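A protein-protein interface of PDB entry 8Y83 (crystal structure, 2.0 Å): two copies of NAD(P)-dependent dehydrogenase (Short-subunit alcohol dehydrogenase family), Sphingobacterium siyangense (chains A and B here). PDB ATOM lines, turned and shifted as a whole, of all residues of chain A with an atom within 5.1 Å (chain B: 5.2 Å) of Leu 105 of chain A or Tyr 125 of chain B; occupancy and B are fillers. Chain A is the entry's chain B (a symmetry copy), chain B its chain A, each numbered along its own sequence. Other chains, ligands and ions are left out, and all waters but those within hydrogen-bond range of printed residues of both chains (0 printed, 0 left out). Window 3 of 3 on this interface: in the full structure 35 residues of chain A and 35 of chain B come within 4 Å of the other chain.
The side-chain amino group of Lys 124 of chain B lies within hydrogen-bond range of the backbone carbonyl oxygen of Tyr 103 of chain A, 2.8 Å away.
Among the printed residues, pairs that only touch across the chains: Trp 108 of chain A with Phe 120 of chain B (3.4 Å), Leu 105 of chain A with Tyr 125 of chain B (3.7 Å), Leu 105 of chain A with Pro 67 of chain B (3.8 Å) and Leu 105 of chain A with Lys 124 of chain B (3.9 Å).
Of the printed residues of chain B, Tyr 103 of chain A touches Lys 124 (2.8 Å). Leu 105 of chain A touches just these residues of chain B: Pro 67, Lys 124 and Tyr 125. Gly 107 of chain A touches none of the printed residues of chain B. Gly 122 of chain B touches none of the printed residues of chain A. Printed residues of chain A within 4 Å of Lys 124 of chain B: Tyr 103 and Leu 105. Of the printed residues of chain A, Tyr 125 of chain B touches Leu 105 (3.7 Å). The nearest printed residue of chain B that does not touch Trp 108 of chain A is Tyr 121 of chain B (4.5 Å).
Of the 14 printed residues of chain B, 4 touch a printed residue of chain A. Printed residues of chain B that touch a printed residue of chain A: Pro 67, Phe 120, Lys 124 and Tyr 125. Hydrophobic or aromatic side chains of chain B that line the printed part of chain A: Pro 67, Phe 120 and Tyr 125. Hydrophobic or aromatic side chains of chain A that line the printed part of chain B: Leu 105 and Trp 108. Among the printed residues, 5 pairs touch across the chains.
No position is printed for both chains. Of the 5 pairs that touch across the chains among the printed residues, none has its exchanged pair printed and touching as well.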
ATOM      1  N   TYR A 103      -2.563 -15.057 -24.382  1.00  0.00           N
ATOM      2  CA  TYR A 103      -1.700 -13.893 -24.456  1.00  0.00           C
ATOM      3  C   TYR A 103      -1.820 -13.098 -23.146  1.00  0.00           C
ATOM      4  O   TYR A 103      -2.921 -12.825 -22.710  1.00  0.00           O
ATOM      5  CB  TYR A 103      -2.023 -13.106 -25.734  1.00  0.00           C
ATOM      6  CG  TYR A 103      -0.786 -12.489 -26.368  1.00  0.00           C
ATOM      7  CD1 TYR A 103      -0.231 -11.317 -25.878  1.00  0.00           C
ATOM      8  CD2 TYR A 103      -0.149 -13.119 -27.434  1.00  0.00           C
ATOM      9  CE1 TYR A 103       0.964 -10.835 -26.395  1.00  0.00           C
ATOM     10  CE2 TYR A 103       1.014 -12.612 -27.991  1.00  0.00           C
ATOM     11  CZ  TYR A 103       1.557 -11.453 -27.481  1.00  0.00           C
ATOM     12  OH  TYR A 103       2.717 -10.992 -28.028  1.00  0.00           O
ATOM     13  N   SER A 104      -0.687 -12.774 -22.493  1.00  0.00           N
ATOM     14  CA  SER A 104      -0.684 -12.047 -21.225  1.00  0.00           C
ATOM     15  C   SER A 104      -1.150 -10.615 -21.470  1.00  0.00           C
ATOM     16  O   SER A 104      -0.852 -10.058 -22.525  1.00  0.00           O
ATOM     17  CB  SER A 104       0.683 -12.076 -20.542  1.00  0.00           C
ATOM     18  OG  SER A 104       1.610 -11.192 -21.141  1.00  0.00           O
ATOM     19  N   LEU A 105      -1.889 -10.040 -20.504  1.00  0.00           N
ATOM     20  CA  LEU A 105      -2.352  -8.661 -20.592  1.00  0.00           C
ATOM     21  C   LEU A 105      -1.188  -7.684 -20.713  1.00  0.00           C
ATOM     22  O   LEU A 105      -1.275  -6.726 -21.478  1.00  0.00           O
ATOM     23  CB  LEU A 105      -3.271  -8.272 -19.441  1.00  0.00           C
ATOM     24  CG  LEU A 105      -4.504  -9.164 -19.305  1.00  0.00           C
ATOM     25  CD1 LEU A 105      -5.377  -8.683 -18.175  1.00  0.00           C
ATOM     26  CD2 LEU A 105      -5.299  -9.220 -20.593  1.00  0.00           C
ATOM     27  N   ASP A 106      -0.096  -7.932 -19.983  1.00  0.00           N
ATOM     28  CA  ASP A 106       1.034  -7.013 -19.952  1.00  0.00           C
ATOM     29  C   ASP A 106       1.820  -7.121 -21.256  1.00  0.00           C
ATOM     30  O   ASP A 106       2.255  -6.100 -21.789  1.00  0.00           O
ATOM     31  CB  ASP A 106       1.901  -7.268 -18.728  1.00  0.00           C
ATOM     32  CG  ASP A 106       2.047  -8.739 -18.379  1.00  0.00           C
ATOM     33  OD1 ASP A 106       0.991  -9.398 -18.142  1.00  0.00           O
ATOM     34  OD2 ASP A 106       3.198  -9.223 -18.370  1.00  0.00           O
ATOM     35  N   GLY A 107       2.036  -8.366 -21.733  1.00  0.00           N
ATOM     36  CA  GLY A 107       2.719  -8.613 -22.995  1.00  0.00           C
ATOM     37  C   GLY A 107       1.951  -7.992 -24.179  1.00  0.00           C
ATOM     38  O   GLY A 107       2.538  -7.423 -25.096  1.00  0.00           O
ATOM     39  N   TRP A 108       0.629  -8.101 -24.139  1.00  0.00           N
ATOM     40  CA  TRP A 108      -0.211  -7.527 -25.177  1.00  0.00           C
ATOM     41  C   TRP A 108       0.039  -6.024 -25.261  1.00  0.00           C
ATOM     42  O   TRP A 108       0.406  -5.514 -26.328  1.00  0.00           O
ATOM     43  CB  TRP A 108      -1.703  -7.826 -24.920  1.00  0.00           C
ATOM     44  CG  TRP A 108      -2.617  -7.131 -25.894  1.00  0.00           C
ATOM     45  CD1 TRP A 108      -3.196  -5.899 -25.789  1.00  0.00           C
ATOM     46  CD2 TRP A 108      -3.034  -7.666 -27.157  1.00  0.00           C
ATOM     47  NE1 TRP A 108      -3.942  -5.629 -26.897  1.00  0.00           N
ATOM     48  CE2 TRP A 108      -3.864  -6.696 -27.755  1.00  0.00           C
ATOM     49  CE3 TRP A 108      -2.801  -8.875 -27.815  1.00  0.00           C
ATOM     50  CZ2 TRP A 108      -4.443  -6.892 -28.995  1.00  0.00           C
ATOM     51  CZ3 TRP A 108      -3.348  -9.048 -29.063  1.00  0.00           C
ATOM     52  CH2 TRP A 108      -4.136  -8.060 -29.647  1.00  0.00           C
ATOM     53  N   LYS A 109      -0.140  -5.350 -24.114  1.00  0.00           N
ATOM     54  CA  LYS A 109      -0.041  -3.902 -24.020  1.00  0.00           C
ATOM     55  C   LYS A 109       1.342  -3.431 -24.454  1.00  0.00           C
ATOM     56  O   LYS A 109       1.466  -2.356 -25.046  1.00  0.00           O
ATOM     57  CB  LYS A 109      -0.417  -3.324 -22.645  1.00  0.00           C
ATOM     58  CG  LYS A 109       0.099  -1.886 -22.400  1.00  0.00           C
ATOM     59  CD  LYS A 109      -0.591  -0.952 -21.400  1.00  0.00           C
ATOM     60  CE  LYS A 109      -1.096   0.367 -21.972  1.00  0.00           C
ATOM     61  NZ  LYS A 109      -2.298   0.277 -22.808  1.00  0.00           N
ATOM     62  N   PRO B  67     -10.307  -5.258 -19.134  1.00  0.00           N
ATOM     63  CA  PRO B  67     -10.091  -6.710 -19.094  1.00  0.00           C
ATOM     64  C   PRO B  67     -10.984  -7.399 -18.051  1.00  0.00           C
ATOM     65  O   PRO B  67     -11.663  -8.379 -18.364  1.00  0.00           O
ATOM     66  CB  PRO B  67      -8.588  -6.821 -18.736  1.00  0.00           C
ATOM     67  CG  PRO B  67      -7.980  -5.497 -19.155  1.00  0.00           C
ATOM     68  CD  PRO B  67      -9.068  -4.481 -18.968  1.00  0.00           C
ATOM     69  N   ASN B  70     -14.600  -7.710 -19.127  1.00  0.00           N
ATOM     70  CA  ASN B  70     -14.807  -8.690 -20.181  1.00  0.00           C
ATOM     71  C   ASN B  70     -14.790 -10.105 -19.587  1.00  0.00           C
ATOM     72  O   ASN B  70     -15.563 -10.980 -19.968  1.00  0.00           O
ATOM     73  CB  ASN B  70     -13.781  -8.554 -21.306  1.00  0.00           C
ATOM     74  CG  ASN B  70     -14.191  -7.512 -22.322  1.00  0.00           C
ATOM     75  OD1 ASN B  70     -15.064  -7.763 -23.147  1.00  0.00           O
ATOM     76  ND2 ASN B  70     -13.566  -6.351 -22.291  1.00  0.00           N
ATOM     77  N   GLU B  71     -13.862 -10.335 -18.676  1.00  0.00           N
ATOM     78  CA  GLU B  71     -13.781 -11.601 -17.981  1.00  0.00           C
ATOM     79  C   GLU B  71     -15.080 -11.823 -17.207  1.00  0.00           C
ATOM     80  O   GLU B  71     -15.684 -12.899 -17.264  1.00  0.00           O
ATOM     81  CB  GLU B  71     -12.530 -11.623 -17.105  1.00  0.00           C
ATOM     82  CG  GLU B  71     -12.335 -12.982 -16.448  1.00  0.00           C
ATOM     83  CD  GLU B  71     -11.091 -13.086 -15.578  1.00  0.00           C
ATOM     84  OE1 GLU B  71     -10.534 -12.058 -15.165  1.00  0.00           O
ATOM     85  OE2 GLU B  71     -10.675 -14.234 -15.337  1.00  0.00           O
ATOM     86  N   VAL B  74     -18.103 -12.694 -19.559  1.00  0.00           N
ATOM     87  CA  VAL B  74     -18.099 -14.077 -20.008  1.00  0.00           C
ATOM     88  C   VAL B  74     -18.503 -14.988 -18.847  1.00  0.00           C
ATOM     89  O   VAL B  74     -19.329 -15.886 -19.048  1.00  0.00           O
ATOM     90  CB  VAL B  74     -16.743 -14.466 -20.613  1.00  0.00           C
ATOM     91  CG1 VAL B  74     -16.684 -15.946 -20.938  1.00  0.00           C
ATOM     92  CG2 VAL B  74     -16.440 -13.628 -21.864  1.00  0.00           C
ATOM     93  N   PHE B 120      -9.808  -7.331 -28.210  1.00  0.00           N
ATOM     94  CA  PHE B 120      -8.896  -8.391 -27.802  1.00  0.00           C
ATOM     95  C   PHE B 120      -9.287  -8.972 -26.426  1.00  0.00           C
ATOM     96  O   PHE B 120      -9.336 -10.188 -26.275  1.00  0.00           O
ATOM     97  CB  PHE B 120      -7.444  -7.915 -27.818  1.00  0.00           C
ATOM     98  CG  PHE B 120      -6.561  -8.801 -26.951  1.00  0.00           C
ATOM     99  CD1 PHE B 120      -6.299 -10.129 -27.301  1.00  0.00           C
ATOM    100  CD2 PHE B 120      -6.052  -8.318 -25.762  1.00  0.00           C
ATOM    101  CE1 PHE B 120      -5.526 -10.936 -26.476  1.00  0.00           C
ATOM    102  CE2 PHE B 120      -5.322  -9.129 -24.929  1.00  0.00           C
ATOM    103  CZ  PHE B 120      -5.038 -10.429 -25.281  1.00  0.00           C
ATOM    104  N   TYR B 121      -9.605  -8.113 -25.445  1.00  0.00           N
ATOM    105  CA  TYR B 121      -9.951  -8.552 -24.099  1.00  0.00           C
ATOM    106  C   TYR B 121     -11.187  -9.456 -24.157  1.00  0.00           C
ATOM    107  O   TYR B 121     -11.184 -10.524 -23.558  1.00  0.00           O
ATOM    108  CB  TYR B 121     -10.214  -7.378 -23.143  1.00  0.00           C
ATOM    109  CG  TYR B 121      -9.041  -6.423 -22.982  1.00  0.00           C
ATOM    110  CD1 TYR B 121      -7.740  -6.903 -23.004  1.00  0.00           C
ATOM    111  CD2 TYR B 121      -9.231  -5.052 -22.830  1.00  0.00           C
ATOM    112  CE1 TYR B 121      -6.656  -6.050 -22.881  1.00  0.00           C
ATOM    113  CE2 TYR B 121      -8.149  -4.183 -22.717  1.00  0.00           C
ATOM    114  CZ  TYR B 121      -6.858  -4.689 -22.741  1.00  0.00           C
ATOM    115  OH  TYR B 121      -5.783  -3.838 -22.652  1.00  0.00           O
ATOM    116  N   GLY B 122     -12.210  -9.024 -24.910  1.00  0.00           N
ATOM    117  CA  GLY B 122     -13.359  -9.848 -25.211  1.00  0.00           C
ATOM    118  C   GLY B 122     -12.962 -11.212 -25.789  1.00  0.00           C
ATOM    119  O   GLY B 122     -13.385 -12.266 -25.290  1.00  0.00           O
ATOM    120  N   CYS B 123     -12.251 -11.192 -26.916  1.00  0.00           N
ATOM    121  CA  CYS B 123     -11.876 -12.420 -27.594  1.00  0.00           C
ATOM    122  C   CYS B 123     -11.143 -13.366 -26.642  1.00  0.00           C
ATOM    123  O   CYS B 123     -11.344 -14.584 -26.696  1.00  0.00           O
ATOM    124  CB  CYS B 123     -11.004 -12.151 -28.823  1.00  0.00           C
ATOM    125  SG  CYS B 123     -11.912 -11.415 -30.227  1.00  0.00           S
ATOM    126  N   LYS B 124     -10.199 -12.823 -25.866  1.00  0.00           N
ATOM    127  CA  LYS B 124      -9.388 -13.633 -24.954  1.00  0.00           C
ATOM    128  C   LYS B 124     -10.284 -14.440 -24.004  1.00  0.00           C
ATOM    129  O   LYS B 124     -10.117 -15.657 -23.890  1.00  0.00           O
ATOM    130  CB  LYS B 124      -8.425 -12.754 -24.151  1.00  0.00           C
ATOM    131  CG  LYS B 124      -7.497 -13.467 -23.142  1.00  0.00           C
ATOM    132  CD  LYS B 124      -6.783 -12.451 -22.263  1.00  0.00           C
ATOM    133  CE  LYS B 124      -6.063 -13.081 -21.095  1.00  0.00           C
ATOM    134  NZ  LYS B 124      -5.114 -14.066 -21.590  1.00  0.00           N
ATOM    135  N   TYR B 125     -11.251 -13.781 -23.354  1.00  0.00           N
ATOM    136  CA  TYR B 125     -12.073 -14.464 -22.351  1.00  0.00           C
ATOM    137  C   TYR B 125     -13.149 -15.298 -23.030  1.00  0.00           C
ATOM    138  O   TYR B 125     -13.535 -16.343 -22.517  1.00  0.00           O
ATOM    139  CB  TYR B 125     -12.595 -13.471 -21.297  1.00  0.00           C
ATOM    140  CG  TYR B 125     -11.422 -12.859 -20.536  1.00  0.00           C
ATOM    141  CD1 TYR B 125     -10.574 -13.645 -19.746  1.00  0.00           C
ATOM    142  CD2 TYR B 125     -11.142 -11.507 -20.623  1.00  0.00           C
ATOM    143  CE1 TYR B 125      -9.477 -13.098 -19.086  1.00  0.00           C
ATOM    144  CE2 TYR B 125     -10.057 -10.949 -19.976  1.00  0.00           C
ATOM    145  CZ  TYR B 125      -9.209 -11.752 -19.235  1.00  0.00           C
ATOM    146  OH  TYR B 125      -8.197 -11.112 -18.629  1.00  0.00           O
ATOM    147  N   GLN B 126     -13.623 -14.850 -24.201  1.00  0.00           N
ATOM    148  CA  GLN B 126     -14.557 -15.641 -24.989  1.00  0.00           C
ATOM    149  C   GLN B 126     -13.921 -16.979 -25.406  1.00  0.00           C
ATOM    150  O   GLN B 126     -14.523 -18.045 -25.289  1.00  0.00           O
ATOM    151  CB  GLN B 126     -15.029 -14.785 -26.157  1.00  0.00           C
ATOM    152  CG  GLN B 126     -15.875 -13.585 -25.745  1.00  0.00           C
ATOM    153  CD  GLN B 126     -15.859 -12.443 -26.752  1.00  0.00           C
ATOM    154  OE1 GLN B 126     -15.392 -12.573 -27.897  1.00  0.00           O
ATOM    155  NE2 GLN B 126     -16.399 -11.304 -26.331  1.00  0.00           N
ATOM    156  N   ILE B 127     -12.709 -16.911 -25.932  1.00  0.00           N
ATOM    157  CA  ILE B 127     -11.969 -18.092 -26.358  1.00  0.00           C
ATOM    158  C   ILE B 127     -11.863 -19.097 -25.206  1.00  0.00           C
ATOM    159  O   ILE B 127     -12.034 -20.302 -25.408  1.00  0.00           O
ATOM    160  CB  ILE B 127     -10.576 -17.662 -26.882  1.00  0.00           C
ATOM    161  CG1 ILE B 127     -10.689 -17.046 -28.302  1.00  0.00           C
ATOM    162  CG2 ILE B 127      -9.578 -18.810 -26.849  1.00  0.00           C
ATOM    163  CD1 ILE B 127      -9.441 -16.312 -28.765  1.00  0.00           C
ATOM    164  N   GLU B 128     -11.538 -18.599 -24.011  1.00  0.00           N
ATOM    165  CA  GLU B 128     -11.382 -19.458 -22.837  1.00  0.00           C
ATOM    166  C   GLU B 128     -12.668 -20.247 -22.581  1.00  0.00           C
ATOM    167  O   GLU B 128     -12.621 -21.472 -22.445  1.00  0.00           O
ATOM    168  CB  GLU B 128     -10.955 -18.632 -21.623  1.00  0.00           C
ATOM    169  CG  GLU B 128     -10.986 -19.412 -20.309  1.00  0.00           C
ATOM    170  CD  GLU B 128     -10.652 -18.578 -19.073  1.00  0.00           C
ATOM    171  OE1 GLU B 128     -11.171 -17.447 -18.927  1.00  0.00           O
ATOM    172  OE2 GLU B 128      -9.875 -19.079 -18.238  1.00  0.00           O
ATOM    173  N   ALA B 129     -13.826 -19.571 -22.640  1.00  0.00           N
ATOM    174  CA  ALA B 129     -15.094 -20.246 -22.434  1.00  0.00           C
ATOM    175  C   ALA B 129     -15.411 -21.210 -23.562  1.00  0.00           C
ATOM    176  O   ALA B 129     -15.823 -22.352 -23.320  1.00  0.00           O
ATOM    177  CB  ALA B 129     -16.176 -19.242 -22.256  1.00  0.00           C
